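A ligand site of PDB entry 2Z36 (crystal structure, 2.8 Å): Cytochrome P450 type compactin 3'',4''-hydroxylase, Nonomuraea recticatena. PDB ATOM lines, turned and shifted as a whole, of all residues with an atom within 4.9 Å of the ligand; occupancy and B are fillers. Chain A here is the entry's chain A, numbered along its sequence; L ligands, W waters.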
ATOM      1  N   MET A  95      28.221  25.065 -10.108  1.00  0.00           N
ATOM      2  CA  MET A  95      26.814  24.852 -10.391  1.00  0.00           C
ATOM      3  C   MET A  95      26.065  26.027  -9.787  1.00  0.00           C
ATOM      4  O   MET A  95      25.089  26.527 -10.335  1.00  0.00           O
ATOM      5  CB  MET A  95      26.343  23.548  -9.753  1.00  0.00           C
ATOM      6  CG  MET A  95      24.846  23.283  -9.876  1.00  0.00           C
ATOM      7  SD  MET A  95      24.434  21.563  -9.539  1.00  0.00           S
ATOM      8  CE  MET A  95      24.438  21.571  -7.826  1.00  0.00           C
ATOM      9  N   LEU A  96      26.565  26.474  -8.636  1.00  0.00           N
ATOM     10  CA  LEU A  96      25.991  27.574  -7.892  1.00  0.00           C
ATOM     11  C   LEU A  96      26.149  28.893  -8.652  1.00  0.00           C
ATOM     12  O   LEU A  96      25.605  29.923  -8.248  1.00  0.00           O
ATOM     13  CB  LEU A  96      26.689  27.639  -6.527  1.00  0.00           C
ATOM     14  CG  LEU A  96      25.970  28.203  -5.310  1.00  0.00           C
ATOM     15  CD1 LEU A  96      24.574  27.627  -5.201  1.00  0.00           C
ATOM     16  CD2 LEU A  96      26.782  27.868  -4.085  1.00  0.00           C
ATOM     17  N   HIS A 103      23.207  25.311 -16.431  1.00  0.00           N
ATOM     18  CA  HIS A 103      22.946  24.875 -15.062  1.00  0.00           C
ATOM     19  C   HIS A 103      22.317  23.488 -15.074  1.00  0.00           C
ATOM     20  O   HIS A 103      22.866  22.533 -14.515  1.00  0.00           O
ATOM     21  CB  HIS A 103      21.997  25.836 -14.347  1.00  0.00           C
ATOM     22  CG  HIS A 103      21.580  25.373 -12.985  1.00  0.00           C
ATOM     23  ND1 HIS A 103      20.281  25.471 -12.520  1.00  0.00           N
ATOM     24  CD2 HIS A 103      22.291  24.805 -11.985  1.00  0.00           C
ATOM     25  CE1 HIS A 103      20.215  24.990 -11.295  1.00  0.00           C
ATOM     26  NE2 HIS A 103      21.420  24.573 -10.937  1.00  0.00           N
ATOM     27  N   ARG A 107      23.257  19.996 -13.202  1.00  0.00           N
ATOM     28  CA  ARG A 107      22.515  19.460 -12.068  1.00  0.00           C
ATOM     29  C   ARG A 107      21.819  18.124 -12.318  1.00  0.00           C
ATOM     30  O   ARG A 107      21.824  17.248 -11.457  1.00  0.00           O
ATOM     31  CB  ARG A 107      21.488  20.480 -11.570  1.00  0.00           C
ATOM     32  CG  ARG A 107      20.822  20.048 -10.290  1.00  0.00           C
ATOM     33  CD  ARG A 107      20.074  21.171  -9.627  1.00  0.00           C
ATOM     34  NE  ARG A 107      19.692  20.793  -8.273  1.00  0.00           N
ATOM     35  CZ  ARG A 107      19.114  21.613  -7.402  1.00  0.00           C
ATOM     36  NH1 ARG A 107      18.850  22.860  -7.735  1.00  0.00           N
ATOM     37  NH2 ARG A 107      18.805  21.179  -6.183  1.00  0.00           N
ATOM     38  N   PHE A 114      20.308  12.111  -4.566  1.00  0.00           N
ATOM     39  CA  PHE A 114      19.566  12.623  -3.411  1.00  0.00           C
ATOM     40  C   PHE A 114      18.083  12.234  -3.362  1.00  0.00           C
ATOM     41  O   PHE A 114      17.277  12.892  -2.704  1.00  0.00           O
ATOM     42  CB  PHE A 114      19.706  14.148  -3.358  1.00  0.00           C
ATOM     43  CG  PHE A 114      21.128  14.612  -3.204  1.00  0.00           C
ATOM     44  CD1 PHE A 114      21.721  14.683  -1.954  1.00  0.00           C
ATOM     45  CD2 PHE A 114      21.899  14.896  -4.332  1.00  0.00           C
ATOM     46  CE1 PHE A 114      23.068  15.041  -1.817  1.00  0.00           C
ATOM     47  CE2 PHE A 114      23.240  15.249  -4.201  1.00  0.00           C
ATOM     48  CZ  PHE A 114      23.828  15.317  -2.942  1.00  0.00           C
ATOM     49  N   ILE A 160      29.236  13.048   4.484  1.00  0.00           N
ATOM     50  CA  ILE A 160      29.519  13.360   3.085  1.00  0.00           C
ATOM     51  C   ILE A 160      30.563  12.433   2.478  1.00  0.00           C
ATOM     52  O   ILE A 160      30.416  12.005   1.334  1.00  0.00           O
ATOM     53  CB  ILE A 160      29.979  14.831   2.913  1.00  0.00           C
ATOM     54  CG1 ILE A 160      28.823  15.773   3.275  1.00  0.00           C
ATOM     55  CG2 ILE A 160      30.424  15.079   1.480  1.00  0.00           C
ATOM     56  CD1 ILE A 160      29.127  17.247   3.054  1.00  0.00           C
ATOM     57  N   LEU A 241      32.421  20.657  -4.223  1.00  0.00           N
ATOM     58  CA  LEU A 241      31.209  21.464  -4.210  1.00  0.00           C
ATOM     59  C   LEU A 241      30.292  20.932  -3.125  1.00  0.00           C
ATOM     60  O   LEU A 241      29.795  21.691  -2.294  1.00  0.00           O
ATOM     61  CB  LEU A 241      30.465  21.393  -5.559  1.00  0.00           C
ATOM     62  CG  LEU A 241      29.113  22.132  -5.583  1.00  0.00           C
ATOM     63  CD1 LEU A 241      29.337  23.621  -5.741  1.00  0.00           C
ATOM     64  CD2 LEU A 241      28.273  21.613  -6.739  1.00  0.00           C
ATOM     65  N   LEU A 242      30.084  19.623  -3.148  1.00  0.00           N
ATOM     66  CA  LEU A 242      29.236  18.946  -2.182  1.00  0.00           C
ATOM     67  C   LEU A 242      29.715  19.139  -0.750  1.00  0.00           C
ATOM     68  O   LEU A 242      28.952  19.576   0.117  1.00  0.00           O
ATOM     69  CB  LEU A 242      29.180  17.448  -2.513  1.00  0.00           C
ATOM     70  CG  LEU A 242      27.901  16.895  -3.163  1.00  0.00           C
ATOM     71  CD1 LEU A 242      27.324  17.898  -4.139  1.00  0.00           C
ATOM     72  CD2 LEU A 242      28.216  15.577  -3.866  1.00  0.00           C
ATOM     73  N   LEU A 243      30.977  18.832  -0.505  1.00  0.00           N
ATOM     74  CA  LEU A 243      31.553  18.978   0.826  1.00  0.00           C
ATOM     75  C   LEU A 243      31.426  20.437   1.266  1.00  0.00           C
ATOM     76  O   LEU A 243      30.960  20.728   2.362  1.00  0.00           O
ATOM     77  CB  LEU A 243      33.037  18.588   0.803  1.00  0.00           C
ATOM     78  CG  LEU A 243      33.798  18.716   2.120  1.00  0.00           C
ATOM     79  CD1 LEU A 243      33.365  17.628   3.073  1.00  0.00           C
ATOM     80  CD2 LEU A 243      35.290  18.617   1.861  1.00  0.00           C
ATOM     81  N   ALA A 245      29.426  23.031   0.164  1.00  0.00           N
ATOM     82  CA  ALA A 245      28.078  23.540   0.394  1.00  0.00           C
ATOM     83  C   ALA A 245      27.271  22.769   1.433  1.00  0.00           C
ATOM     84  O   ALA A 245      26.161  23.179   1.764  1.00  0.00           O
ATOM     85  CB  ALA A 245      27.312  23.583  -0.917  1.00  0.00           C
ATOM     86  N   GLY A 246      27.832  21.678   1.951  1.00  0.00           N
ATOM     87  CA  GLY A 246      27.076  20.907   2.925  1.00  0.00           C
ATOM     88  C   GLY A 246      27.721  20.597   4.269  1.00  0.00           C
ATOM     89  O   GLY A 246      27.074  19.997   5.126  1.00  0.00           O
ATOM     90  N   THR A 249      27.325  24.466   6.738  1.00  0.00           N
ATOM     91  CA  THR A 249      25.900  24.764   6.848  1.00  0.00           C
ATOM     92  C   THR A 249      25.224  23.772   7.787  1.00  0.00           C
ATOM     93  O   THR A 249      24.531  24.160   8.726  1.00  0.00           O
ATOM     94  CB  THR A 249      25.190  24.677   5.479  1.00  0.00           C
ATOM     95  OG1 THR A 249      25.552  23.452   4.831  1.00  0.00           O
ATOM     96  CG2 THR A 249      25.572  25.854   4.613  1.00  0.00           C
ATOM     97  N   THR A 250      25.446  22.488   7.545  1.00  0.00           N
ATOM     98  CA  THR A 250      24.873  21.453   8.376  1.00  0.00           C
ATOM     99  C   THR A 250      25.410  21.561   9.793  1.00  0.00           C
ATOM    100  O   THR A 250      24.649  21.568  10.762  1.00  0.00           O
ATOM    101  CB  THR A 250      25.207  20.053   7.837  1.00  0.00           C
ATOM    102  OG1 THR A 250      24.781  19.946   6.476  1.00  0.00           O
ATOM    103  CG2 THR A 250      24.501  18.983   8.661  1.00  0.00           C
ATOM    104  N   MET A 253      23.914  24.257  11.594  1.00  0.00           N
ATOM    105  CA  MET A 253      22.508  23.956  11.835  1.00  0.00           C
ATOM    106  C   MET A 253      22.361  23.026  13.030  1.00  0.00           C
ATOM    107  O   MET A 253      21.383  23.102  13.775  1.00  0.00           O
ATOM    108  CB  MET A 253      21.887  23.321  10.603  1.00  0.00           C
ATOM    109  CG  MET A 253      21.051  24.291   9.801  1.00  0.00           C
ATOM    110  SD  MET A 253      19.893  25.139  10.890  1.00  0.00           S
ATOM    111  CE  MET A 253      20.012  26.768  10.293  1.00  0.00           C
ATOM    112  N   ILE A 291      20.343  30.287   8.472  1.00  0.00           N
ATOM    113  CA  ILE A 291      21.769  30.589   8.453  1.00  0.00           C
ATOM    114  C   ILE A 291      22.428  30.919   7.104  1.00  0.00           C
ATOM    115  O   ILE A 291      23.622  31.211   7.054  1.00  0.00           O
ATOM    116  CB  ILE A 291      22.573  29.430   9.072  1.00  0.00           C
ATOM    117  CG1 ILE A 291      22.366  28.164   8.238  1.00  0.00           C
ATOM    118  CG2 ILE A 291      22.134  29.214  10.521  1.00  0.00           C
ATOM    119  CD1 ILE A 291      23.163  26.975   8.712  1.00  0.00           C
ATOM    120  N   ALA A 292      21.658  30.884   6.021  1.00  0.00           N
ATOM    121  CA  ALA A 292      22.237  31.199   4.712  1.00  0.00           C
ATOM    122  C   ALA A 292      21.769  32.577   4.252  1.00  0.00           C
ATOM    123  O   ALA A 292      22.067  33.009   3.141  1.00  0.00           O
ATOM    124  CB  ALA A 292      21.837  30.127   3.703  1.00  0.00           C
ATOM    125  N   VAL A 295      23.237  34.668   1.062  1.00  0.00           N
ATOM    126  CA  VAL A 295      24.114  34.056   0.073  1.00  0.00           C
ATOM    127  C   VAL A 295      23.422  34.084  -1.279  1.00  0.00           C
ATOM    128  O   VAL A 295      24.062  33.842  -2.308  1.00  0.00           O
ATOM    129  CB  VAL A 295      24.441  32.582   0.408  1.00  0.00           C
ATOM    130  CG1 VAL A 295      25.202  32.499   1.726  1.00  0.00           C
ATOM    131  CG2 VAL A 295      23.166  31.750   0.473  1.00  0.00           C
ATOM    132  N   THR A 296      22.123  34.378  -1.285  1.00  0.00           N
ATOM    133  CA  THR A 296      21.368  34.428  -2.533  1.00  0.00           C
ATOM    134  C   THR A 296      21.412  35.789  -3.219  1.00  0.00           C
ATOM    135  O   THR A 296      20.395  36.494  -3.321  1.00  0.00           O
ATOM    136  CB  THR A 296      19.882  34.041  -2.305  1.00  0.00           C
ATOM    137  OG1 THR A 296      19.364  34.749  -1.171  1.00  0.00           O
ATOM    138  CG2 THR A 296      19.752  32.545  -2.068  1.00  0.00           C
ATOM    139  N   ARG A 298      21.989  38.081  -6.576  1.00  0.00           N
ATOM    140  CA  ARG A 298      21.735  37.877  -8.001  1.00  0.00           C
ATOM    141  C   ARG A 298      22.083  39.112  -8.820  1.00  0.00           C
ATOM    142  O   ARG A 298      22.257  40.208  -8.279  1.00  0.00           O
ATOM    143  CB  ARG A 298      20.265  37.518  -8.216  1.00  0.00           C
ATOM    144  CG  ARG A 298      19.840  36.180  -7.608  1.00  0.00           C
ATOM    145  CD  ARG A 298      20.320  35.010  -8.446  1.00  0.00           C
ATOM    146  NE  ARG A 298      19.911  33.724  -7.897  1.00  0.00           N
ATOM    147  CZ  ARG A 298      20.358  33.225  -6.755  1.00  0.00           C
ATOM    148  NH1 ARG A 298      21.239  33.902  -6.029  1.00  0.00           N
ATOM    149  NH2 ARG A 298      19.930  32.043  -6.325  1.00  0.00           N
ATOM    150  N   MET A 321      16.866  35.658   2.707  1.00  0.00           N
ATOM    151  CA  MET A 321      16.063  34.529   3.140  1.00  0.00           C
ATOM    152  C   MET A 321      15.607  34.650   4.596  1.00  0.00           C
ATOM    153  O   MET A 321      14.468  34.331   4.923  1.00  0.00           O
ATOM    154  CB  MET A 321      16.828  33.229   2.916  1.00  0.00           C
ATOM    155  CG  MET A 321      17.110  32.980   1.441  1.00  0.00           C
ATOM    156  SD  MET A 321      17.989  31.449   1.126  1.00  0.00           S
ATOM    157  CE  MET A 321      19.689  31.996   1.320  1.00  0.00           C
ATOM    158  N   ALA A 348      14.886  28.745   3.796  1.00  0.00           N
ATOM    159  CA  ALA A 348      16.232  28.478   4.299  1.00  0.00           C
ATOM    160  C   ALA A 348      17.063  27.671   3.307  1.00  0.00           C
ATOM    161  O   ALA A 348      18.293  27.724   3.312  1.00  0.00           O
ATOM    162  CB  ALA A 348      16.156  27.758   5.635  1.00  0.00           C
ATOM    163  N   PHE A 349      16.388  26.908   2.442  1.00  0.00           N
ATOM    164  CA  PHE A 349      17.063  26.089   1.448  1.00  0.00           C
ATOM    165  C   PHE A 349      17.023  26.758   0.085  1.00  0.00           C
ATOM    166  O   PHE A 349      17.467  26.193  -0.921  1.00  0.00           O
ATOM    167  CB  PHE A 349      16.392  24.720   1.347  1.00  0.00           C
ATOM    168  CG  PHE A 349      16.861  23.734   2.378  1.00  0.00           C
ATOM    169  CD1 PHE A 349      15.940  22.934   3.065  1.00  0.00           C
ATOM    170  CD2 PHE A 349      18.209  23.568   2.649  1.00  0.00           C
ATOM    171  CE1 PHE A 349      16.367  22.001   3.995  1.00  0.00           C
ATOM    172  CE2 PHE A 349      18.654  22.624   3.587  1.00  0.00           C
ATOM    173  CZ  PHE A 349      17.727  21.843   4.264  1.00  0.00           C
ATOM    174  N   GLY A 350      16.492  27.970   0.034  1.00  0.00           N
ATOM    175  CA  GLY A 350      16.395  28.664  -1.232  1.00  0.00           C
ATOM    176  C   GLY A 350      15.122  28.278  -1.946  1.00  0.00           C
ATOM    177  O   GLY A 350      14.268  27.580  -1.392  1.00  0.00           O
ATOM    178  N   PRO A 353      15.463  27.095  -9.424  1.00  0.00           N
ATOM    179  CA  PRO A 353      16.454  26.225 -10.062  1.00  0.00           C
ATOM    180  C   PRO A 353      17.620  25.816  -9.174  1.00  0.00           C
ATOM    181  O   PRO A 353      18.098  24.684  -9.237  1.00  0.00           O
ATOM    182  CB  PRO A 353      16.930  27.056 -11.258  1.00  0.00           C
ATOM    183  CG  PRO A 353      15.749  27.894 -11.574  1.00  0.00           C
ATOM    184  CD  PRO A 353      15.280  28.327 -10.208  1.00  0.00           C
ATOM    185  N   HIS A 354      18.081  26.743  -8.341  1.00  0.00           N
ATOM    186  CA  HIS A 354      19.217  26.485  -7.472  1.00  0.00           C
ATOM    187  C   HIS A 354      18.888  26.005  -6.065  1.00  0.00           C
ATOM    188  O   HIS A 354      19.787  25.865  -5.248  1.00  0.00           O
ATOM    189  CB  HIS A 354      20.090  27.734  -7.395  1.00  0.00           C
ATOM    190  CG  HIS A 354      20.802  28.051  -8.671  1.00  0.00           C
ATOM    191  ND1 HIS A 354      21.783  27.243  -9.190  1.00  0.00           N
ATOM    192  CD2 HIS A 354      20.664  29.079  -9.535  1.00  0.00           C
ATOM    193  CE1 HIS A 354      22.213  27.752 -10.330  1.00  0.00           C
ATOM    194  NE2 HIS A 354      21.552  28.867 -10.564  1.00  0.00           N
ATOM    195  N   GLN A 355      17.615  25.743  -5.789  1.00  0.00           N
ATOM    196  CA  GLN A 355      17.251  25.288  -4.451  1.00  0.00           C
ATOM    197  C   GLN A 355      18.220  24.191  -4.024  1.00  0.00           C
ATOM    198  O   GLN A 355      18.660  23.382  -4.837  1.00  0.00           O
ATOM    199  CB  GLN A 355      15.819  24.761  -4.415  1.00  0.00           C
ATOM    200  CG  GLN A 355      15.288  24.610  -2.997  1.00  0.00           C
ATOM    201  CD  GLN A 355      13.943  23.923  -2.956  1.00  0.00           C
ATOM    202  OE1 GLN A 355      13.774  22.849  -3.538  1.00  0.00           O
ATOM    203  NE2 GLN A 355      12.987  24.516  -2.264  1.00  0.00           N
ATOM    204  N   CYS A 356      18.548  24.165  -2.732  1.00  0.00           N
ATOM    205  CA  CYS A 356      19.501  23.213  -2.185  1.00  0.00           C
ATOM    206  C   CYS A 356      19.391  21.793  -2.708  1.00  0.00           C
ATOM    207  O   CYS A 356      18.353  21.144  -2.569  1.00  0.00           O
ATOM    208  CB  CYS A 356      19.427  23.209  -0.663  1.00  0.00           C
ATOM    209  SG  CYS A 356      20.712  22.191   0.078  1.00  0.00           S
ATOM    210  N   LEU A 357      20.475  21.308  -3.305  1.00  0.00           N
ATOM    211  CA  LEU A 357      20.514  19.966  -3.858  1.00  0.00           C
ATOM    212  C   LEU A 357      20.522  18.896  -2.756  1.00  0.00           C
ATOM    213  O   LEU A 357      19.913  17.838  -2.904  1.00  0.00           O
ATOM    214  CB  LEU A 357      21.774  19.801  -4.713  1.00  0.00           C
ATOM    215  CG  LEU A 357      21.793  18.861  -5.922  1.00  0.00           C
ATOM    216  CD1 LEU A 357      23.184  18.242  -6.020  1.00  0.00           C
ATOM    217  CD2 LEU A 357      20.750  17.771  -5.794  1.00  0.00           C
ATOM    218  N   GLY A 358      21.217  19.178  -1.650  1.00  0.00           N
ATOM    219  CA  GLY A 358      21.282  18.208  -0.573  1.00  0.00           C
ATOM    220  C   GLY A 358      20.390  18.540   0.601  1.00  0.00           C
ATOM    221  O   GLY A 358      20.600  18.066   1.720  1.00  0.00           O
ATOM    222  N   GLN A 359      19.359  19.347   0.345  1.00  0.00           N
ATOM    223  CA  GLN A 359      18.424  19.763   1.376  1.00  0.00           C
ATOM    224  C   GLN A 359      17.798  18.574   2.112  1.00  0.00           C
ATOM    225  O   GLN A 359      17.449  18.676   3.290  1.00  0.00           O
ATOM    226  CB  GLN A 359      17.314  20.633   0.789  1.00  0.00           C
ATOM    227  CG  GLN A 359      16.407  19.918  -0.204  1.00  0.00           C
ATOM    228  CD  GLN A 359      15.475  20.869  -0.930  1.00  0.00           C
ATOM    229  OE1 GLN A 359      14.342  21.117  -0.507  1.00  0.00           O
ATOM    230  NE2 GLN A 359      15.958  21.423  -2.028  1.00  0.00           N
ATOM    231  N   LEU A 361      19.326  15.503   2.369  1.00  0.00           N
ATOM    232  CA  LEU A 361      20.368  14.764   3.071  1.00  0.00           C
ATOM    233  C   LEU A 361      20.551  15.507   4.384  1.00  0.00           C
ATOM    234  O   LEU A 361      20.795  14.909   5.431  1.00  0.00           O
ATOM    235  CB  LEU A 361      21.674  14.768   2.287  1.00  0.00           C
ATOM    236  CG  LEU A 361      22.890  14.226   3.047  1.00  0.00           C
ATOM    237  CD1 LEU A 361      22.602  12.818   3.536  1.00  0.00           C
ATOM    238  CD2 LEU A 361      24.109  14.247   2.138  1.00  0.00           C
ATOM    239  N   ALA A 362      20.423  16.832   4.309  1.00  0.00           N
ATOM    240  CA  ALA A 362      20.559  17.690   5.473  1.00  0.00           C
ATOM    241  C   ALA A 362      19.434  17.390   6.464  1.00  0.00           C
ATOM    242  O   ALA A 362      19.673  17.158   7.641  1.00  0.00           O
ATOM    243  CB  ALA A 362      20.519  19.148   5.058  1.00  0.00           C
ATOM    244  N   GLU A 365      20.142  14.173   8.227  1.00  0.00           N
ATOM    245  CA  GLU A 365      21.205  14.294   9.233  1.00  0.00           C
ATOM    246  C   GLU A 365      20.684  14.948  10.512  1.00  0.00           C
ATOM    247  O   GLU A 365      20.813  14.397  11.595  1.00  0.00           O
ATOM    248  CB  GLU A 365      22.377  15.110   8.684  1.00  0.00           C
ATOM    249  CG  GLU A 365      23.383  14.313   7.890  1.00  0.00           C
ATOM    250  CD  GLU A 365      24.402  15.208   7.207  1.00  0.00           C
ATOM    251  OE1 GLU A 365      24.032  15.889   6.227  1.00  0.00           O
ATOM    252  OE2 GLU A 365      25.568  15.226   7.657  1.00  0.00           O
HETATM  253  C1  LIG L   1      22.515  25.270  -2.712  1.00  0.00           C
HETATM  254  C2  LIG L   1      21.282  25.963   1.798  1.00  0.00           C
HETATM  255  C3  LIG L   1      23.075  21.742   2.981  1.00  0.00           C
HETATM  256  C4  LIG L   1      24.255  20.980  -1.566  1.00  0.00           C
HETATM  257  C5  LIG L   1      21.986  25.806  -1.585  1.00  0.00           C
HETATM  258  C6  LIG L   1      21.288  27.043  -1.516  1.00  0.00           C
HETATM  259  C7  LIG L   1      20.975  27.250  -0.234  1.00  0.00           C
HETATM  260  C8  LIG L   1      21.451  26.131   0.483  1.00  0.00           C
HETATM  261  C9  LIG L   1      20.231  28.438   0.353  1.00  0.00           C
HETATM  262  C10 LIG L   1      20.968  27.989  -2.686  1.00  0.00           C
HETATM  263  C11 LIG L   1      22.040  29.080  -2.857  1.00  0.00           C
HETATM  264  C12 LIG L   1      21.708  29.996  -4.008  1.00  0.00           C
HETATM  265  O1  LIG L   1      20.707  29.839  -4.672  1.00  0.00           O
HETATM  266  O2  LIG L   1      22.536  31.013  -4.322  1.00  0.00           O
HETATM  267  C13 LIG L   1      21.718  24.890   2.515  1.00  0.00           C
HETATM  268  C14 LIG L   1      21.534  24.813   3.930  1.00  0.00           C
HETATM  269  C15 LIG L   1      22.024  23.653   4.331  1.00  0.00           C
HETATM  270  C16 LIG L   1      22.539  22.997   3.060  1.00  0.00           C
HETATM  271  C17 LIG L   1      20.892  25.873   4.803  1.00  0.00           C
HETATM  272  C18 LIG L   1      22.012  23.167   5.749  1.00  0.00           C
HETATM  273  C19 LIG L   1      22.496  21.991   6.153  1.00  0.00           C
HETATM  274  C20 LIG L   1      23.529  21.150   1.843  1.00  0.00           C
HETATM  275  C21 LIG L   1      24.030  19.822   1.778  1.00  0.00           C
HETATM  276  C22 LIG L   1      24.384  19.592   0.479  1.00  0.00           C
HETATM  277  C23 LIG L   1      24.080  20.809  -0.243  1.00  0.00           C
HETATM  278  C24 LIG L   1      24.148  18.855   2.947  1.00  0.00           C
HETATM  279  C25 LIG L   1      24.960  18.336  -0.088  1.00  0.00           C
HETATM  280  C26 LIG L   1      26.221  17.975   0.138  1.00  0.00           C
HETATM  281  C27 LIG L   1      23.935  22.146  -2.229  1.00  0.00           C
HETATM  282  C28 LIG L   1      24.235  22.338  -3.672  1.00  0.00           C
HETATM  283  C29 LIG L   1      23.746  23.523  -3.998  1.00  0.00           C
HETATM  284  C30 LIG L   1      23.161  24.076  -2.751  1.00  0.00           C
HETATM  285  C31 LIG L   1      24.945  21.361  -4.568  1.00  0.00           C
HETATM  286  C32 LIG L   1      23.770  24.203  -5.349  1.00  0.00           C
HETATM  287  C33 LIG L   1      22.456  23.895  -6.091  1.00  0.00           C
HETATM  288  C34 LIG L   1      22.404  24.556  -7.452  1.00  0.00           C
HETATM  289  O3  LIG L   1      23.323  25.237  -7.860  1.00  0.00           O
HETATM  290  O4  LIG L   1      21.321  24.385  -8.220  1.00  0.00           O
HETATM  291  N1  LIG L   1      22.105  25.225  -0.338  1.00  0.00           N
HETATM  292  N2  LIG L   1      22.370  23.836   2.014  1.00  0.00           N
HETATM  293  N3  LIG L   1      23.560  21.754   0.613  1.00  0.00           N
HETATM  294  N4  LIG L   1      23.370  23.240  -1.714  1.00  0.00           N
HETATM  295 FE1  LIG L   1      22.960  23.536   0.164  1.00  0.00          FE
HETATM  296  O   HOH W   1      17.970  29.426  -4.194  1.00  0.00           O
HETATM  297  O   HOH W   2      19.229  28.634   5.756  1.00  0.00           O
HETATM  298  O   HOH W   3      24.755  31.583  -3.220  1.00  0.00           O
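O4 of the ligand is in salt-bridge range of NH1 of Arg 107 (2.9 Å). An oxygen (O3) of the ligand sits at hydrogen-bond distance from a ring nitrogen (ND1) of His 354, 2.9 Å away. An oxygen (O4) of the ligand lies within hydrogen-bond range of a ring nitrogen (NE2) of His 103 (2.7 Å). The guanidinium group (NH2) of Arg 298 lies within salt-bridge range of an oxygen (O1) of the ligand. The side-chain sulfur (SG) of Cys 356 binds an iron atom (FE1) of the ligand.
NE2 of Gln 355 is in hydrogen-bond range of O of Gly 350, 3.4 Å away. OG1 of Thr 250 is in hydrogen-bond range of O of Gly 246 (2.7 Å). O of Gln 355 lies within hydrogen-bond range of NH2 of Arg 107, at 2.6 Å. The backbone carbonyl oxygen (O) of Cys 356 lies within hydrogen-bond range of the side-chain amide nitrogen (NE2) of Gln 359, 2.5 Å away. SG of Cys 356 sits close to N of Gly 358 (3.5 Å). NE2 of His 103 sits at hydrogen-bond distance from ND1 of His 354, 3.2 Å away. The backbone carbonyl oxygen (O) of Pro 353 is in hydrogen-bond range of the guanidinium group (NH1) of Arg 107, 2.5 Å away. The backbone carbonyl oxygen of Ala 245 lies within hydrogen-bond range of the side-chain hydroxyl of Thr 249 (3.1 Å).
An oxygen (O3) of the ligand lies close to the backbone carbonyl oxygen of Met 95. A nitrogen (N3) of the ligand lies close to the backbone carbonyl oxygen (O) of Ala 245 (3.2 Å). The backbone carbonyl oxygen of Pro 353 sits close to an oxygen (O4) of the ligand, 3.4 Å away. Leu 96 touches the ligand (CD1 to C32, 3.5 Å). Leu 241 touches the ligand. Leu 242 touches the ligand (O to C26, 3.2 Å). CA of Gly 246 touches C21 of the ligand, 3.4 Å away. Thr 249 touches the ligand (CB to C15, 3.5 Å). OG1 of Thr 250 touches C19 of the ligand (3.1 Å). Val 295 touches the ligand (O to O2, 3.8 Å). Thr 296 touches the ligand (CG2 to C12, 3.8 Å). Met 321 touches the ligand (CE to C9, 3.7 Å). O of Ala 348 touches C17 of the ligand (3.5 Å). Phe 349 touches the ligand (CE2 to C15, 3.6 Å). Gly 350 touches the ligand (N to C9, 3.8 Å). Leu 357 touches the ligand. Gly 358 touches the ligand. Ala 362 touches the ligand. Hydrophobic or aromatic side chains within 4 Å of the ligand: Met 95, Leu 96, His 103, Leu 241, Leu 242, Ala 245, Met 321, Phe 349, His 354, Leu 357 and Ala 362. Of the 33 residues printed, 23 come within 4 Å of the ligand. The nearest printed residue that does not touch the ligand is Gln 355 (4.03 Å).
Water W3 bridges the backbone carbonyl oxygen of Val 295 (2.5 Å) and an oxygen (O2) of the ligand (2.5 Å). Water W2 lies within hydrogen-bond range of the backbone carbonyl oxygen (O) of Ala 348 (2.8 Å), the backbone NH (N) of Ala 292 (3.3 Å) and the backbone NH (N) of Ile 291 (3.4 Å).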
